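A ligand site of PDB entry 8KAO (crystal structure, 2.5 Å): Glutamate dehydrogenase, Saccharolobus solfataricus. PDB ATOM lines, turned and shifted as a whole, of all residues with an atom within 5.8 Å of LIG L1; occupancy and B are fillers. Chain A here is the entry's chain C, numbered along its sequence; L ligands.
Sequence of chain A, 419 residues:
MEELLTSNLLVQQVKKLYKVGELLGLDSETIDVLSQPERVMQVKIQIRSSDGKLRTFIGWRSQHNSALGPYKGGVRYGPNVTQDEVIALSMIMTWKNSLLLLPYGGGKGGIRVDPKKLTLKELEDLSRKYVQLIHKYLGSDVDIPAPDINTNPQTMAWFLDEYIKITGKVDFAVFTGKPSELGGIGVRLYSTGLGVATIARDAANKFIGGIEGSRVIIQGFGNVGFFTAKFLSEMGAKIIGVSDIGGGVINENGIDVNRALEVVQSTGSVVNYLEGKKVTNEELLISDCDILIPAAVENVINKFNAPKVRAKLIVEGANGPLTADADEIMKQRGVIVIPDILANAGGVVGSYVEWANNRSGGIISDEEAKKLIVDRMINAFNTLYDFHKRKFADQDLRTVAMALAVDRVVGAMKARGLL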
ATOM      1  N   LYS A  72      10.454  10.708   7.894  1.00  0.00           N
ATOM      2  CA  LYS A  72      10.526   9.557   7.003  1.00  0.00           C
ATOM      3  C   LYS A  72      11.683   8.655   7.403  1.00  0.00           C
ATOM      4  O   LYS A  72      12.786   9.142   7.689  1.00  0.00           O
ATOM      5  CB  LYS A  72      10.794  10.003   5.562  1.00  0.00           C
ATOM      6  CG  LYS A  72      10.627   8.905   4.522  1.00  0.00           C
ATOM      7  CD  LYS A  72       9.186   8.687   4.167  1.00  0.00           C
ATOM      8  CE  LYS A  72       8.891   7.398   3.432  1.00  0.00           C
ATOM      9  NZ  LYS A  72       8.884   6.230   4.337  1.00  0.00           N
ATOM     10  N   GLY A  73      11.459   7.336   7.354  1.00  0.00           N
ATOM     11  CA  GLY A  73      12.573   6.402   7.359  1.00  0.00           C
ATOM     12  C   GLY A  73      12.232   5.058   7.980  1.00  0.00           C
ATOM     13  O   GLY A  73      11.210   4.925   8.661  1.00  0.00           O
ATOM     14  N   GLY A  74      13.164   4.104   7.800  1.00  0.00           N
ATOM     15  CA  GLY A  74      12.946   2.705   8.099  1.00  0.00           C
ATOM     16  C   GLY A  74      12.962   2.361   9.583  1.00  0.00           C
ATOM     17  O   GLY A  74      13.249   3.201  10.433  1.00  0.00           O
ATOM     18  N   VAL A  75      12.614   1.098   9.857  1.00  0.00           N
ATOM     19  CA  VAL A  75      12.667   0.487  11.177  1.00  0.00           C
ATOM     20  C   VAL A  75      13.592  -0.726  11.112  1.00  0.00           C
ATOM     21  O   VAL A  75      13.311  -1.640  10.311  1.00  0.00           O
ATOM     22  CB  VAL A  75      11.252  -0.004  11.595  1.00  0.00           C
ATOM     23  CG1 VAL A  75      11.288  -0.688  12.960  1.00  0.00           C
ATOM     24  CG2 VAL A  75      10.210   1.102  11.542  1.00  0.00           C
ATOM     25  N   MET A  93      18.755  10.334   7.852  1.00  0.00           N
ATOM     26  CA  MET A  93      17.542  10.471   7.040  1.00  0.00           C
ATOM     27  C   MET A  93      17.314  11.947   6.728  1.00  0.00           C
ATOM     28  O   MET A  93      17.120  12.332   5.576  1.00  0.00           O
ATOM     29  CB  MET A  93      16.290   9.947   7.750  1.00  0.00           C
ATOM     30  CG  MET A  93      16.226   8.451   7.883  1.00  0.00           C
ATOM     31  SD  MET A  93      16.670   7.585   6.351  1.00  0.00           S
ATOM     32  CE  MET A  93      15.399   8.163   5.237  1.00  0.00           C
ATOM     33  N   LYS A  96      19.625  12.973   3.981  1.00  0.00           N
ATOM     34  CA  LYS A  96      19.335  12.205   2.784  1.00  0.00           C
ATOM     35  C   LYS A  96      18.100  12.775   2.095  1.00  0.00           C
ATOM     36  O   LYS A  96      18.061  12.965   0.883  1.00  0.00           O
ATOM     37  CB  LYS A  96      19.120  10.743   3.218  1.00  0.00           C
ATOM     38  CG  LYS A  96      19.294   9.659   2.158  1.00  0.00           C
ATOM     39  CD  LYS A  96      18.540   8.389   2.481  1.00  0.00           C
ATOM     40  CE  LYS A  96      18.841   7.761   3.833  1.00  0.00           C
ATOM     41  NZ  LYS A  96      19.747   6.603   3.745  1.00  0.00           N
ATOM     42  N   GLY A 107      13.456  10.448  10.195  1.00  0.00           N
ATOM     43  CA  GLY A 107      13.067   9.609  11.298  1.00  0.00           C
ATOM     44  C   GLY A 107      13.547   8.192  11.041  1.00  0.00           C
ATOM     45  O   GLY A 107      13.956   7.874   9.917  1.00  0.00           O
ATOM     46  N   LYS A 108      13.572   7.385  12.105  1.00  0.00           N
ATOM     47  CA  LYS A 108      13.897   5.977  11.995  1.00  0.00           C
ATOM     48  C   LYS A 108      13.352   5.302  13.230  1.00  0.00           C
ATOM     49  O   LYS A 108      13.120   5.959  14.233  1.00  0.00           O
ATOM     50  CB  LYS A 108      15.417   5.726  11.894  1.00  0.00           C
ATOM     51  CG  LYS A 108      15.934   5.368  10.511  1.00  0.00           C
ATOM     52  CD  LYS A 108      16.513   3.979  10.440  1.00  0.00           C
ATOM     53  CE  LYS A 108      16.751   3.442   9.051  1.00  0.00           C
ATOM     54  NZ  LYS A 108      16.954   4.504   8.035  1.00  0.00           N
ATOM     55  N   PRO A 145       7.050   5.287   8.200  1.00  0.00           N
ATOM     56  CA  PRO A 145       8.129   4.298   8.263  1.00  0.00           C
ATOM     57  C   PRO A 145       8.290   3.483   6.987  1.00  0.00           C
ATOM     58  O   PRO A 145       7.614   3.718   5.992  1.00  0.00           O
ATOM     59  CB  PRO A 145       7.756   3.378   9.424  1.00  0.00           C
ATOM     60  CG  PRO A 145       6.661   4.110  10.180  1.00  0.00           C
ATOM     61  CD  PRO A 145       5.969   4.989   9.151  1.00  0.00           C
ATOM     62  N   ALA A 146       9.267   2.555   7.028  1.00  0.00           N
ATOM     63  CA  ALA A 146       9.634   1.727   5.889  1.00  0.00           C
ATOM     64  C   ALA A 146      10.562   0.621   6.369  1.00  0.00           C
ATOM     65  O   ALA A 146      10.908   0.552   7.566  1.00  0.00           O
ATOM     66  CB  ALA A 146      10.314   2.566   4.839  1.00  0.00           C
ATOM     67  N   PRO A 147      10.983  -0.291   5.464  1.00  0.00           N
ATOM     68  CA  PRO A 147      11.854  -1.393   5.877  1.00  0.00           C
ATOM     69  C   PRO A 147      13.282  -0.905   6.154  1.00  0.00           C
ATOM     70  O   PRO A 147      13.756   0.083   5.570  1.00  0.00           O
ATOM     71  CB  PRO A 147      11.814  -2.365   4.654  1.00  0.00           C
ATOM     72  CG  PRO A 147      10.579  -1.923   3.881  1.00  0.00           C
ATOM     73  CD  PRO A 147      10.574  -0.421   4.059  1.00  0.00           C
ATOM     74  N   ASP A 148      13.969  -1.627   7.052  1.00  0.00           N
ATOM     75  CA  ASP A 148      15.390  -1.459   7.252  1.00  0.00           C
ATOM     76  C   ASP A 148      15.986  -2.864   7.393  1.00  0.00           C
ATOM     77  O   ASP A 148      15.596  -3.781   6.649  1.00  0.00           O
ATOM     78  CB  ASP A 148      15.677  -0.545   8.443  1.00  0.00           C
ATOM     79  CG  ASP A 148      17.105  -0.025   8.460  1.00  0.00           C
ATOM     80  OD1 ASP A 148      17.411   0.881   7.672  1.00  0.00           O
ATOM     81  OD2 ASP A 148      17.913  -0.548   9.248  1.00  0.00           O
ATOM     82  N   THR A 176       5.868   2.693   3.753  1.00  0.00           N
ATOM     83  CA  THR A 176       6.421   2.480   2.418  1.00  0.00           C
ATOM     84  C   THR A 176       7.211   1.175   2.422  1.00  0.00           C
ATOM     85  O   THR A 176       7.391   0.560   3.475  1.00  0.00           O
ATOM     86  CB  THR A 176       7.294   3.658   1.954  1.00  0.00           C
ATOM     87  OG1 THR A 176       8.238   4.065   2.977  1.00  0.00           O
ATOM     88  CG2 THR A 176       6.423   4.844   1.547  1.00  0.00           C
ATOM     89  N   ARG A 188      10.357  -0.759  -5.546  1.00  0.00           N
ATOM     90  CA  ARG A 188      10.817  -0.445  -4.203  1.00  0.00           C
ATOM     91  C   ARG A 188      11.609  -1.619  -3.630  1.00  0.00           C
ATOM     92  O   ARG A 188      12.538  -1.411  -2.843  1.00  0.00           O
ATOM     93  CB  ARG A 188       9.621  -0.043  -3.343  1.00  0.00           C
ATOM     94  CG  ARG A 188      10.018   0.307  -1.920  1.00  0.00           C
ATOM     95  CD  ARG A 188      11.063   1.409  -1.839  1.00  0.00           C
ATOM     96  NE  ARG A 188      11.521   1.579  -0.468  1.00  0.00           N
ATOM     97  CZ  ARG A 188      12.616   1.007   0.006  1.00  0.00           C
ATOM     98  NH1 ARG A 188      13.359   0.277  -0.811  1.00  0.00           N
ATOM     99  NH2 ARG A 188      12.949   1.147   1.281  1.00  0.00           N
ATOM    100  N   THR A 192      16.891   0.473  -3.630  1.00  0.00           N
ATOM    101  CA  THR A 192      18.101   0.876  -2.935  1.00  0.00           C
ATOM    102  C   THR A 192      19.323   0.343  -3.671  1.00  0.00           C
ATOM    103  O   THR A 192      20.198   1.132  -3.996  1.00  0.00           O
ATOM    104  CB  THR A 192      18.121   0.445  -1.478  1.00  0.00           C
ATOM    105  OG1 THR A 192      16.867   0.795  -0.913  1.00  0.00           O
ATOM    106  CG2 THR A 192      19.219   1.143  -0.710  1.00  0.00           C
ATOM    107  N   ASN A 319      23.857   2.782   5.856  1.00  0.00           N
ATOM    108  CA  ASN A 319      23.820   4.055   6.581  1.00  0.00           C
ATOM    109  C   ASN A 319      24.998   4.110   7.542  1.00  0.00           C
ATOM    110  O   ASN A 319      25.186   3.192   8.333  1.00  0.00           O
ATOM    111  CB  ASN A 319      22.518   4.203   7.372  1.00  0.00           C
ATOM    112  CG  ASN A 319      21.315   4.360   6.468  1.00  0.00           C
ATOM    113  OD1 ASN A 319      21.210   5.373   5.794  1.00  0.00           O
ATOM    114  ND2 ASN A 319      20.433   3.377   6.439  1.00  0.00           N
ATOM    115  N   ASN A 344      22.516   5.459  -1.004  1.00  0.00           N
ATOM    116  CA  ASN A 344      21.443   4.543  -0.646  1.00  0.00           C
ATOM    117  C   ASN A 344      20.078   5.214  -0.716  1.00  0.00           C
ATOM    118  O   ASN A 344      19.082   4.654  -0.254  1.00  0.00           O
ATOM    119  CB  ASN A 344      21.694   3.959   0.747  1.00  0.00           C
ATOM    120  CG  ASN A 344      21.025   4.756   1.847  1.00  0.00           C
ATOM    121  OD1 ASN A 344      21.514   5.807   2.249  1.00  0.00           O
ATOM    122  ND2 ASN A 344      19.906   4.238   2.344  1.00  0.00           N
ATOM    123  N   ALA A 345      20.022   6.390  -1.318  1.00  0.00           N
ATOM    124  CA  ALA A 345      18.761   7.131  -1.406  1.00  0.00           C
ATOM    125  C   ALA A 345      17.751   6.458  -2.319  1.00  0.00           C
ATOM    126  O   ALA A 345      16.566   6.753  -2.230  1.00  0.00           O
ATOM    127  CB  ALA A 345      19.031   8.557  -1.840  1.00  0.00           C
ATOM    128  N   GLY A 347      16.388   3.943  -1.928  1.00  0.00           N
ATOM    129  CA  GLY A 347      15.352   3.483  -1.017  1.00  0.00           C
ATOM    130  C   GLY A 347      14.281   4.544  -0.833  1.00  0.00           C
ATOM    131  O   GLY A 347      13.134   4.344  -1.219  1.00  0.00           O
ATOM    132  N   VAL A 348      14.700   5.691  -0.289  1.00  0.00           N
ATOM    133  CA  VAL A 348      13.786   6.731   0.134  1.00  0.00           C
ATOM    134  C   VAL A 348      13.145   7.385  -1.082  1.00  0.00           C
ATOM    135  O   VAL A 348      12.003   7.857  -1.025  1.00  0.00           O
ATOM    136  CB  VAL A 348      14.486   7.817   0.968  1.00  0.00           C
ATOM    137  CG1 VAL A 348      13.545   8.369   2.038  1.00  0.00           C
ATOM    138  CG2 VAL A 348      15.773   7.302   1.576  1.00  0.00           C
ATOM    139  N   SER A 351      10.523   5.166  -2.151  1.00  0.00           N
ATOM    140  CA  SER A 351       9.361   5.147  -1.280  1.00  0.00           C
ATOM    141  C   SER A 351       8.650   6.505  -1.296  1.00  0.00           C
ATOM    142  O   SER A 351       7.433   6.577  -1.096  1.00  0.00           O
ATOM    143  CB  SER A 351       9.752   4.646   0.110  1.00  0.00           C
ATOM    144  OG  SER A 351      10.064   5.708   0.980  1.00  0.00           O
HETATM  145  C1  LIG L   1      12.252   4.562   2.936  1.00  0.00           C
HETATM  146  C2  LIG L   1      13.149   4.723   4.155  1.00  0.00           C
HETATM  147  C3  LIG L   1      14.462   4.089   3.753  1.00  0.00           C
HETATM  148  C4  LIG L   1      15.462   4.188   4.922  1.00  0.00           C
HETATM  149  O1  LIG L   1      15.145   4.220   6.134  1.00  0.00           O
HETATM  150  C5  LIG L   1      16.938   4.347   4.553  1.00  0.00           C
HETATM  151  O2  LIG L   1      17.281   4.444   3.307  1.00  0.00           O
HETATM  152  O3  LIG L   1      17.790   4.453   5.513  1.00  0.00           O
HETATM  153  P1  LG2 L   2      18.860  -6.785   5.261  1.00  0.00           P
HETATM  154  O1  LG2 L   2      18.302  -7.151   6.606  1.00  0.00           O
HETATM  155  O2  LG2 L   2      18.064  -7.004   4.012  1.00  0.00           O
HETATM  156  O3  LG2 L   2      20.268  -7.506   5.061  1.00  0.00           O
HETATM  157  C1  LG2 L   2      21.317  -7.311   6.010  1.00  0.00           C
HETATM  158  C2  LG2 L   2      22.543  -7.938   5.407  1.00  0.00           C
HETATM  159  O4  LG2 L   2      23.706  -7.500   6.144  1.00  0.00           O
HETATM  160  C3  LG2 L   2      22.568  -9.470   5.478  1.00  0.00           C
HETATM  161  O5  LG2 L   2      23.415 -10.038   4.488  1.00  0.00           O
HETATM  162  C4  LG2 L   2      23.216  -9.677   6.840  1.00  0.00           C
HETATM  163  O6  LG2 L   2      23.667 -11.012   7.028  1.00  0.00           O
HETATM  164  C5  LG2 L   2      24.310  -8.632   6.731  1.00  0.00           C
HETATM  165  N1  LG2 L   2      24.891  -8.249   8.018  1.00  0.00           N
HETATM  166  C6  LG2 L   2      24.221  -8.083   9.202  1.00  0.00           C
HETATM  167  N2  LG2 L   2      25.017  -7.816  10.217  1.00  0.00           N
HETATM  168  C7  LG2 L   2      26.291  -7.801   9.653  1.00  0.00           C
HETATM  169  C8  LG2 L   2      27.562  -7.563  10.184  1.00  0.00           C
HETATM  170  N3  LG2 L   2      27.773  -7.269  11.465  1.00  0.00           N
HETATM  171  N4  LG2 L   2      28.634  -7.596   9.355  1.00  0.00           N
HETATM  172  C9  LG2 L   2      28.422  -7.892   8.060  1.00  0.00           C
HETATM  173  N5  LG2 L   2      27.265  -8.142   7.438  1.00  0.00           N
HETATM  174  C10 LG2 L   2      26.225  -8.074   8.293  1.00  0.00           C
HETATM  175  O7  LG2 L   2      19.260  -5.248   5.429  1.00  0.00           O
HETATM  176  P2  LG2 L   2      19.361  -4.130   4.291  1.00  0.00           P
HETATM  177  O8  LG2 L   2      17.984  -3.578   4.093  1.00  0.00           O
HETATM  178  O9  LG2 L   2      20.132  -4.734   3.143  1.00  0.00           O
HETATM  179  O10 LG2 L   2      20.290  -3.043   5.034  1.00  0.00           O
HETATM  180  C11 LG2 L   2      21.535  -2.670   4.383  1.00  0.00           C
HETATM  181  C12 LG2 L   2      21.896  -1.251   4.752  1.00  0.00           C
HETATM  182  O11 LG2 L   2      21.109  -0.309   3.968  1.00  0.00           O
HETATM  183  C13 LG2 L   2      21.672  -0.927   6.238  1.00  0.00           C
HETATM  184  O12 LG2 L   2      22.736  -0.177   6.797  1.00  0.00           O
HETATM  185  C14 LG2 L   2      20.351  -0.160   6.231  1.00  0.00           C
HETATM  186  O13 LG2 L   2      20.296   0.835   7.236  1.00  0.00           O
HETATM  187  C15 LG2 L   2      20.313   0.487   4.837  1.00  0.00           C
HETATM  188  N6  LG2 L   2      18.879   0.554   4.405  1.00  0.00           N
HETATM  189  C16 LG2 L   2      18.295  -0.320   3.494  1.00  0.00           C
HETATM  190  C17 LG2 L   2      16.927  -0.191   3.202  1.00  0.00           C
HETATM  191  C18 LG2 L   2      16.114  -0.974   2.229  1.00  0.00           C
HETATM  192  O14 LG2 L   2      14.998  -1.409   2.572  1.00  0.00           O
HETATM  193  N7  LG2 L   2      16.530  -1.068   0.973  1.00  0.00           N
HETATM  194  C19 LG2 L   2      16.157   0.777   3.839  1.00  0.00           C
HETATM  195  C20 LG2 L   2      16.750   1.603   4.765  1.00  0.00           C
HETATM  196  C21 LG2 L   2      18.094   1.476   5.052  1.00  0.00           C
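An oxygen (O1) of LIG L1 lies within hydrogen-bond range of the backbone NH of Gly 74, at 2.6 Å. The side-chain amino group (NZ) of Lys 108 lies within salt-bridge range of an oxygen (O3) of LIG L1 (2.7 Å). The side-chain amide nitrogen of Asn 344 lies within hydrogen-bond range of an oxygen (O2) of LIG L1 (2.8 Å). The side-chain amide nitrogen (ND2) of Asn 319 is in hydrogen-bond range of an oxygen (O3) of LIG L1. The side-chain amino group (NZ) of Lys 96 is in salt-bridge range of an oxygen (O2) of LIG L1, 3.3 Å away. An oxygen (O12) of LG2 L2 is in hydrogen-bond range of the backbone NH of Asn 319 (3.3 Å). The side-chain amide nitrogen of Asn 319 lies within hydrogen-bond range of an oxygen (O13) of LG2 L2. OD1 of Asp 148 sits close to O13 of LG2 L2. N7 of LG2 L2 lies within hydrogen-bond range of OG1 of Thr 192, 2.7 Å away.
The side-chain amino group (NZ) of Lys 108 is in hydrogen-bond range of the side-chain sulfur (SD) of Met 93 (3.5 Å). NZ of Lys 108 lies within salt-bridge range of OD1 of Asp 148 (3.7 Å). The side-chain amide oxygen (OD1) of Asn 344 is in hydrogen-bond range of the side-chain amino group (NZ) of Lys 96, 2.4 Å away. OD1 of Asn 319 lies within hydrogen-bond range of NZ of Lys 96 (2.8 Å). OG of Ser 351 lies within hydrogen-bond range of OG1 of Thr 176 (3.2 Å). N of Ala 146 is in hydrogen-bond range of O of Gly 73, at 3.5 Å. The backbone carbonyl oxygen (O) of Ala 146 is in hydrogen-bond range of the backbone NH (N) of Val 75 (2.9 Å). NE of Arg 188 is in hydrogen-bond range of O of Gly 347, at 3.3 Å.
The side-chain sulfur of Met 93 lies close to an oxygen (O3) of LIG L1 (3.4 Å). Gly 73 touches LIG L1 (C to O1, 3.5 Å). CB of Ala 146 touches C1 of LIG L1, at 3.4 Å. Arg 188 touches LIG L1 (NH2 to C1, 3.9 Å). Val 348 touches LIG L1 (CG2 to O2, 3.7 Å). Ser 351 touches LIG L1. Hydrophobic or aromatic side chains that line LIG L1: Met 93, Ala 146 and Val 348. Within 4 Å of LIG L1: Gly 73, Gly 74, Met 93, Lys 96, Lys 108, Ala 146, Arg 188, Asn 319, Asn 344, Val 348 and Ser 351.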
